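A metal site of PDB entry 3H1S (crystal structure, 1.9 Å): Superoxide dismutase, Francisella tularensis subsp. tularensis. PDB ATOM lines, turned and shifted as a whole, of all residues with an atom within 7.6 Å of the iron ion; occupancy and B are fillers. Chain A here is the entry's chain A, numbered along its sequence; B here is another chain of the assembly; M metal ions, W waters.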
ATOM      1  N   HIS A  30     -15.070 -24.857   8.225  1.00  0.00           N
ATOM      2  CA  HIS A  30     -13.927 -24.042   8.554  1.00  0.00           C
ATOM      3  C   HIS A  30     -12.911 -24.840   9.333  1.00  0.00           C
ATOM      4  O   HIS A  30     -11.777 -24.957   8.955  1.00  0.00           O
ATOM      5  CB  HIS A  30     -14.373 -22.812   9.321  1.00  0.00           C
ATOM      6  CG  HIS A  30     -13.391 -21.692   9.278  1.00  0.00           C
ATOM      7  ND1 HIS A  30     -13.642 -20.484   9.879  1.00  0.00           N
ATOM      8  CD2 HIS A  30     -12.171 -21.587   8.726  1.00  0.00           C
ATOM      9  CE1 HIS A  30     -12.612 -19.689   9.683  1.00  0.00           C
ATOM     10  NE2 HIS A  30     -11.715 -20.330   8.985  1.00  0.00           N
ATOM     11  N   TYR A  31     -13.338 -25.421  10.424  1.00  0.00           N
ATOM     12  CA  TYR A  31     -12.439 -26.205  11.246  1.00  0.00           C
ATOM     13  C   TYR A  31     -12.186 -27.590  10.628  1.00  0.00           C
ATOM     14  O   TYR A  31     -11.042 -28.029  10.467  1.00  0.00           O
ATOM     15  CB  TYR A  31     -13.016 -26.330  12.675  1.00  0.00           C
ATOM     16  CG  TYR A  31     -12.238 -27.283  13.556  1.00  0.00           C
ATOM     17  CD1 TYR A  31     -11.063 -26.874  14.183  1.00  0.00           C
ATOM     18  CD2 TYR A  31     -12.681 -28.580  13.771  1.00  0.00           C
ATOM     19  CE1 TYR A  31     -10.342 -27.731  14.986  1.00  0.00           C
ATOM     20  CE2 TYR A  31     -11.965 -29.448  14.593  1.00  0.00           C
ATOM     21  CZ  TYR A  31     -10.798 -29.022  15.184  1.00  0.00           C
ATOM     22  OH  TYR A  31     -10.081 -29.871  15.970  1.00  0.00           O
ATOM     23  N   HIS A  34     -11.127 -26.812   6.182  1.00  0.00           N
ATOM     24  CA  HIS A  34     -10.124 -25.794   5.837  1.00  0.00           C
ATOM     25  C   HIS A  34      -8.932 -25.978   6.778  1.00  0.00           C
ATOM     26  O   HIS A  34      -7.837 -26.260   6.319  1.00  0.00           O
ATOM     27  CB  HIS A  34     -10.623 -24.344   5.920  1.00  0.00           C
ATOM     28  CG  HIS A  34     -11.592 -23.930   4.837  1.00  0.00           C
ATOM     29  ND1 HIS A  34     -11.197 -23.298   3.676  1.00  0.00           N
ATOM     30  CD2 HIS A  34     -12.942 -23.988   4.796  1.00  0.00           C
ATOM     31  CE1 HIS A  34     -12.268 -23.018   2.946  1.00  0.00           C
ATOM     32  NE2 HIS A  34     -13.356 -23.425   3.608  1.00  0.00           N
ATOM     33  N   HIS A  35      -9.164 -25.858   8.079  1.00  0.00           N
ATOM     34  CA  HIS A  35      -8.087 -26.027   9.085  1.00  0.00           C
ATOM     35  C   HIS A  35      -7.324 -27.343   8.886  1.00  0.00           C
ATOM     36  O   HIS A  35      -6.078 -27.372   8.862  1.00  0.00           O
ATOM     37  CB  HIS A  35      -8.643 -25.949  10.515  1.00  0.00           C
ATOM     38  CG  HIS A  35      -7.652 -25.527  11.571  1.00  0.00           C
ATOM     39  ND1 HIS A  35      -6.297 -25.380  11.337  1.00  0.00           N
ATOM     40  CD2 HIS A  35      -7.832 -25.270  12.880  1.00  0.00           C
ATOM     41  CE1 HIS A  35      -5.701 -25.024  12.469  1.00  0.00           C
ATOM     42  NE2 HIS A  35      -6.615 -24.949  13.411  1.00  0.00           N
ATOM     43  N   TYR A  38      -4.883 -27.426   5.831  1.00  0.00           N
ATOM     44  CA  TYR A  38      -3.633 -26.736   6.078  1.00  0.00           C
ATOM     45  C   TYR A  38      -2.696 -27.685   6.859  1.00  0.00           C
ATOM     46  O   TYR A  38      -1.526 -27.772   6.532  1.00  0.00           O
ATOM     47  CB  TYR A  38      -3.863 -25.458   6.844  1.00  0.00           C
ATOM     48  CG  TYR A  38      -4.620 -24.373   6.077  1.00  0.00           C
ATOM     49  CD1 TYR A  38      -4.136 -23.876   4.844  1.00  0.00           C
ATOM     50  CD2 TYR A  38      -5.759 -23.805   6.590  1.00  0.00           C
ATOM     51  CE1 TYR A  38      -4.790 -22.868   4.165  1.00  0.00           C
ATOM     52  CE2 TYR A  38      -6.435 -22.766   5.886  1.00  0.00           C
ATOM     53  CZ  TYR A  38      -5.943 -22.319   4.684  1.00  0.00           C
ATOM     54  OH  TYR A  38      -6.582 -21.301   3.973  1.00  0.00           O
ATOM     55  N   GLN A  73      -1.240 -20.510   8.320  1.00  0.00           N
ATOM     56  CA  GLN A  73      -2.702 -20.774   8.455  1.00  0.00           C
ATOM     57  C   GLN A  73      -3.072 -21.735   9.568  1.00  0.00           C
ATOM     58  O   GLN A  73      -4.133 -21.590  10.214  1.00  0.00           O
ATOM     59  CB  GLN A  73      -3.299 -21.268   7.145  1.00  0.00           C
ATOM     60  CG  GLN A  73      -3.412 -20.162   6.080  1.00  0.00           C
ATOM     61  CD  GLN A  73      -4.399 -19.040   6.439  1.00  0.00           C
ATOM     62  OE1 GLN A  73      -4.067 -18.121   7.184  1.00  0.00           O
ATOM     63  NE2 GLN A  73      -5.579 -19.086   5.849  1.00  0.00           N
ATOM     64  N   ASN A  76      -2.662 -19.573  12.663  1.00  0.00           N
ATOM     65  CA  ASN A  76      -3.671 -18.519  12.679  1.00  0.00           C
ATOM     66  C   ASN A  76      -5.055 -19.080  13.062  1.00  0.00           C
ATOM     67  O   ASN A  76      -5.777 -18.503  13.884  1.00  0.00           O
ATOM     68  CB  ASN A  76      -3.721 -17.821  11.296  1.00  0.00           C
ATOM     69  CG  ASN A  76      -2.463 -17.014  10.955  1.00  0.00           C
ATOM     70  OD1 ASN A  76      -1.575 -16.818  11.791  1.00  0.00           O
ATOM     71  ND2 ASN A  76      -2.386 -16.559   9.700  1.00  0.00           N
ATOM     72  N   HIS A  77      -5.416 -20.230  12.518  1.00  0.00           N
ATOM     73  CA  HIS A  77      -6.733 -20.796  12.794  1.00  0.00           C
ATOM     74  C   HIS A  77      -6.843 -21.306  14.222  1.00  0.00           C
ATOM     75  O   HIS A  77      -7.848 -21.077  14.851  1.00  0.00           O
ATOM     76  CB  HIS A  77      -7.129 -21.897  11.808  1.00  0.00           C
ATOM     77  CG  HIS A  77      -7.544 -21.401  10.464  1.00  0.00           C
ATOM     78  ND1 HIS A  77      -6.649 -21.266   9.422  1.00  0.00           N
ATOM     79  CD2 HIS A  77      -8.745 -20.945  10.014  1.00  0.00           C
ATOM     80  CE1 HIS A  77      -7.296 -20.804   8.371  1.00  0.00           C
ATOM     81  NE2 HIS A  77      -8.564 -20.603   8.695  1.00  0.00           N
ATOM     82  N   TYR A  80      -7.291 -18.232  16.299  1.00  0.00           N
ATOM     83  CA  TYR A  80      -8.686 -17.760  16.157  1.00  0.00           C
ATOM     84  C   TYR A  80      -9.661 -18.583  17.027  1.00  0.00           C
ATOM     85  O   TYR A  80     -10.462 -18.003  17.778  1.00  0.00           O
ATOM     86  CB  TYR A  80      -9.040 -17.826  14.671  1.00  0.00           C
ATOM     87  CG  TYR A  80     -10.445 -17.559  14.232  1.00  0.00           C
ATOM     88  CD1 TYR A  80     -10.977 -16.282  14.251  1.00  0.00           C
ATOM     89  CD2 TYR A  80     -11.235 -18.576  13.697  1.00  0.00           C
ATOM     90  CE1 TYR A  80     -12.260 -16.043  13.773  1.00  0.00           C
ATOM     91  CE2 TYR A  80     -12.504 -18.347  13.223  1.00  0.00           C
ATOM     92  CZ  TYR A  80     -13.019 -17.092  13.250  1.00  0.00           C
ATOM     93  OH  TYR A  80     -14.270 -16.857  12.751  1.00  0.00           O
ATOM     94  N   TRP A  81      -9.622 -19.905  16.947  1.00  0.00           N
ATOM     95  CA  TRP A  81     -10.577 -20.707  17.743  1.00  0.00           C
ATOM     96  C   TRP A  81     -10.475 -20.407  19.226  1.00  0.00           C
ATOM     97  O   TRP A  81     -11.497 -20.343  19.916  1.00  0.00           O
ATOM     98  CB  TRP A  81     -10.407 -22.212  17.526  1.00  0.00           C
ATOM     99  CG  TRP A  81     -10.503 -22.647  16.147  1.00  0.00           C
ATOM    100  CD1 TRP A  81      -9.575 -23.349  15.469  1.00  0.00           C
ATOM    101  CD2 TRP A  81     -11.575 -22.375  15.211  1.00  0.00           C
ATOM    102  NE1 TRP A  81      -9.982 -23.540  14.171  1.00  0.00           N
ATOM    103  CE2 TRP A  81     -11.203 -22.962  13.986  1.00  0.00           C
ATOM    104  CE3 TRP A  81     -12.791 -21.690  15.289  1.00  0.00           C
ATOM    105  CZ2 TRP A  81     -12.008 -22.890  12.842  1.00  0.00           C
ATOM    106  CZ3 TRP A  81     -13.592 -21.659  14.158  1.00  0.00           C
ATOM    107  CH2 TRP A  81     -13.199 -22.240  12.954  1.00  0.00           C
ATOM    108  N   GLY A 124      -7.817 -12.460   4.524  1.00  0.00           N
ATOM    109  CA  GLY A 124      -6.829 -12.080   5.505  1.00  0.00           C
ATOM    110  C   GLY A 124      -7.354 -12.105   6.924  1.00  0.00           C
ATOM    111  O   GLY A 124      -8.325 -12.798   7.223  1.00  0.00           O
ATOM    112  N   TRP A 125      -6.692 -11.314   7.775  1.00  0.00           N
ATOM    113  CA  TRP A 125      -6.857 -11.340   9.229  1.00  0.00           C
ATOM    114  C   TRP A 125      -6.662  -9.979   9.840  1.00  0.00           C
ATOM    115  O   TRP A 125      -5.807  -9.208   9.423  1.00  0.00           O
ATOM    116  CB  TRP A 125      -5.784 -12.250   9.875  1.00  0.00           C
ATOM    117  CG  TRP A 125      -5.733 -13.642   9.342  1.00  0.00           C
ATOM    118  CD1 TRP A 125      -5.097 -14.087   8.183  1.00  0.00           C
ATOM    119  CD2 TRP A 125      -6.355 -14.788   9.926  1.00  0.00           C
ATOM    120  NE1 TRP A 125      -5.305 -15.438   8.053  1.00  0.00           N
ATOM    121  CE2 TRP A 125      -6.062 -15.877   9.101  1.00  0.00           C
ATOM    122  CE3 TRP A 125      -7.103 -14.992  11.107  1.00  0.00           C
ATOM    123  CZ2 TRP A 125      -6.554 -17.167   9.387  1.00  0.00           C
ATOM    124  CZ3 TRP A 125      -7.575 -16.246  11.382  1.00  0.00           C
ATOM    125  CH2 TRP A 125      -7.296 -17.330  10.518  1.00  0.00           C
ATOM    126  N   ASP A 159     -10.565 -13.858  11.678  1.00  0.00           N
ATOM    127  CA  ASP A 159     -10.451 -14.355  10.326  1.00  0.00           C
ATOM    128  C   ASP A 159     -11.474 -13.652   9.459  1.00  0.00           C
ATOM    129  O   ASP A 159     -12.680 -13.772   9.697  1.00  0.00           O
ATOM    130  CB  ASP A 159     -10.726 -15.865  10.327  1.00  0.00           C
ATOM    131  CG  ASP A 159     -10.327 -16.555   9.025  1.00  0.00           C
ATOM    132  OD1 ASP A 159      -9.902 -15.827   8.116  1.00  0.00           O
ATOM    133  OD2 ASP A 159     -10.442 -17.830   8.910  1.00  0.00           O
ATOM    134  N   VAL A 160     -11.016 -12.960   8.414  1.00  0.00           N
ATOM    135  CA  VAL A 160     -11.939 -12.303   7.425  1.00  0.00           C
ATOM    136  C   VAL A 160     -11.811 -12.865   5.983  1.00  0.00           C
ATOM    137  O   VAL A 160     -12.331 -12.257   4.985  1.00  0.00           O
ATOM    138  CB  VAL A 160     -11.795 -10.750   7.406  1.00  0.00           C
ATOM    139  CG1 VAL A 160     -12.227 -10.174   8.773  1.00  0.00           C
ATOM    140  CG2 VAL A 160     -10.371 -10.252   7.007  1.00  0.00           C
ATOM    141  N   TRP A 161     -11.161 -14.034   5.866  1.00  0.00           N
ATOM    142  CA  TRP A 161     -11.346 -14.883   4.671  1.00  0.00           C
ATOM    143  C   TRP A 161     -12.842 -15.131   4.538  1.00  0.00           C
ATOM    144  O   TRP A 161     -13.525 -15.378   5.549  1.00  0.00           O
ATOM    145  CB  TRP A 161     -10.672 -16.244   4.796  1.00  0.00           C
ATOM    146  CG  TRP A 161      -9.185 -16.277   4.595  1.00  0.00           C
ATOM    147  CD1 TRP A 161      -8.249 -15.639   5.371  1.00  0.00           C
ATOM    148  CD2 TRP A 161      -8.451 -17.030   3.608  1.00  0.00           C
ATOM    149  NE1 TRP A 161      -7.001 -15.939   4.915  1.00  0.00           N
ATOM    150  CE2 TRP A 161      -7.082 -16.791   3.843  1.00  0.00           C
ATOM    151  CE3 TRP A 161      -8.823 -17.860   2.542  1.00  0.00           C
ATOM    152  CZ2 TRP A 161      -6.077 -17.364   3.052  1.00  0.00           C
ATOM    153  CZ3 TRP A 161      -7.829 -18.427   1.756  1.00  0.00           C
ATOM    154  CH2 TRP A 161      -6.478 -18.188   2.028  1.00  0.00           C
ATOM    155  N   GLU A 162     -13.360 -15.086   3.308  1.00  0.00           N
ATOM    156  CA  GLU A 162     -14.805 -15.214   3.086  1.00  0.00           C
ATOM    157  C   GLU A 162     -15.358 -16.549   3.646  1.00  0.00           C
ATOM    158  O   GLU A 162     -16.465 -16.585   4.171  1.00  0.00           O
ATOM    159  CB  GLU A 162     -15.156 -15.021   1.597  1.00  0.00           C
ATOM    160  CG  GLU A 162     -14.994 -13.617   1.143  1.00  0.00           C
ATOM    161  CD  GLU A 162     -15.336 -13.370  -0.266  1.00  0.00           C
ATOM    162  OE1 GLU A 162     -16.082 -12.390  -0.567  1.00  0.00           O
ATOM    163  OE2 GLU A 162     -14.794 -14.082  -1.102  1.00  0.00           O
ATOM    164  N   HIS A 163     -14.584 -17.633   3.587  1.00  0.00           N
ATOM    165  CA  HIS A 163     -15.047 -18.875   4.193  1.00  0.00           C
ATOM    166  C   HIS A 163     -15.449 -18.736   5.697  1.00  0.00           C
ATOM    167  O   HIS A 163     -16.221 -19.525   6.168  1.00  0.00           O
ATOM    168  CB  HIS A 163     -14.074 -20.088   3.997  1.00  0.00           C
ATOM    169  CG  HIS A 163     -12.741 -19.944   4.656  1.00  0.00           C
ATOM    170  ND1 HIS A 163     -11.552 -19.974   3.947  1.00  0.00           N
ATOM    171  CD2 HIS A 163     -12.397 -19.884   5.973  1.00  0.00           C
ATOM    172  CE1 HIS A 163     -10.542 -19.895   4.803  1.00  0.00           C
ATOM    173  NE2 HIS A 163     -11.036 -19.823   6.036  1.00  0.00           N
ATOM    174  N   ALA A 164     -14.857 -17.783   6.425  1.00  0.00           N
ATOM    175  CA  ALA A 164     -15.106 -17.610   7.856  1.00  0.00           C
ATOM    176  C   ALA A 164     -16.560 -17.259   8.155  1.00  0.00           C
ATOM    177  O   ALA A 164     -17.101 -17.571   9.251  1.00  0.00           O
ATOM    178  CB  ALA A 164     -14.203 -16.520   8.379  1.00  0.00           C
ATOM    179  N   TYR A 176     -21.075 -10.042  10.438  1.00  0.00           N
ATOM    180  CA  TYR A 176     -20.133 -11.016  11.026  1.00  0.00           C
ATOM    181  C   TYR A 176     -19.175 -10.397  12.047  1.00  0.00           C
ATOM    182  O   TYR A 176     -19.105 -10.843  13.185  1.00  0.00           O
ATOM    183  CB  TYR A 176     -19.355 -11.703   9.915  1.00  0.00           C
ATOM    184  CG  TYR A 176     -18.118 -12.452  10.320  1.00  0.00           C
ATOM    185  CD1 TYR A 176     -18.189 -13.662  10.981  1.00  0.00           C
ATOM    186  CD2 TYR A 176     -16.831 -11.983   9.949  1.00  0.00           C
ATOM    187  CE1 TYR A 176     -17.032 -14.365  11.346  1.00  0.00           C
ATOM    188  CE2 TYR A 176     -15.686 -12.689  10.270  1.00  0.00           C
ATOM    189  CZ  TYR A 176     -15.787 -13.894  10.973  1.00  0.00           C
ATOM    190  OH  TYR A 176     -14.650 -14.612  11.290  1.00  0.00           O
ATOM    191  N   GLU B 162     -13.507 -16.757  -2.901  1.00  0.00           N
ATOM    192  CA  GLU B 162     -14.414 -17.742  -2.394  1.00  0.00           C
ATOM    193  C   GLU B 162     -15.875 -17.430  -2.686  1.00  0.00           C
ATOM    194  O   GLU B 162     -16.649 -18.337  -2.936  1.00  0.00           O
ATOM    195  CB  GLU B 162     -14.189 -17.961  -0.878  1.00  0.00           C
ATOM    196  CG  GLU B 162     -12.826 -18.683  -0.656  1.00  0.00           C
ATOM    197  CD  GLU B 162     -12.451 -18.892   0.809  1.00  0.00           C
ATOM    198  OE1 GLU B 162     -11.961 -19.989   1.132  1.00  0.00           O
ATOM    199  OE2 GLU B 162     -12.607 -17.947   1.604  1.00  0.00           O
HETATM  200 FE    FE M   1     -10.070 -19.422   7.864  1.00  0.00          FE
HETATM  201  O   HOH W   1      -8.501 -18.211   6.858  1.00  0.00           O
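Water W1 lies within hydrogen-bond range of the side-chain carboxylate (OD1) of Asp 159 (3.0 Å), the side-chain amide nitrogen (NE2) of Gln 73 (3.2 Å) and the indole nitrogen (NE1) of Trp 161 (3.3 Å).
The iron ion is bound by OD2 of Asp 159, NE2 of His 77, NE2 of His 163, NE2 of His 30 and water W1.
The iron ion has five donor atoms within binding distance.
Four residues have an atom within 4 Å of the iron ion: His 30, His 77, Asp 159 and His 163.
The backbone carbonyl oxygen (O) of Gln 73 is in hydrogen-bond range of a ring nitrogen (ND1) of His 77, 2.7 Å away.
O of His 77 sits close to NE1 of Trp 81.
A ring nitrogen (ND1) of His 163 sits close to a ring nitrogen (ND1) of His 34, at 3.4 Å.
The backbone carbonyl oxygen of Asp 159 sits at hydrogen-bond distance from the side-chain hydroxyl of Tyr 176 (2.7 Å).
The backbone NH (N) of His 163 is in hydrogen-bond range of the side-chain carboxylate (OE2) of Glu 162 of chain B, at 2.8 Å.
The side-chain carboxylate (OD1) of Asp 159 sits at hydrogen-bond distance from the backbone NH (N) of Trp 161 (3.1 Å).
The backbone carbonyl oxygen (O) of His 30 lies within hydrogen-bond range of the backbone NH (N) of His 35, 2.9 Å away.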
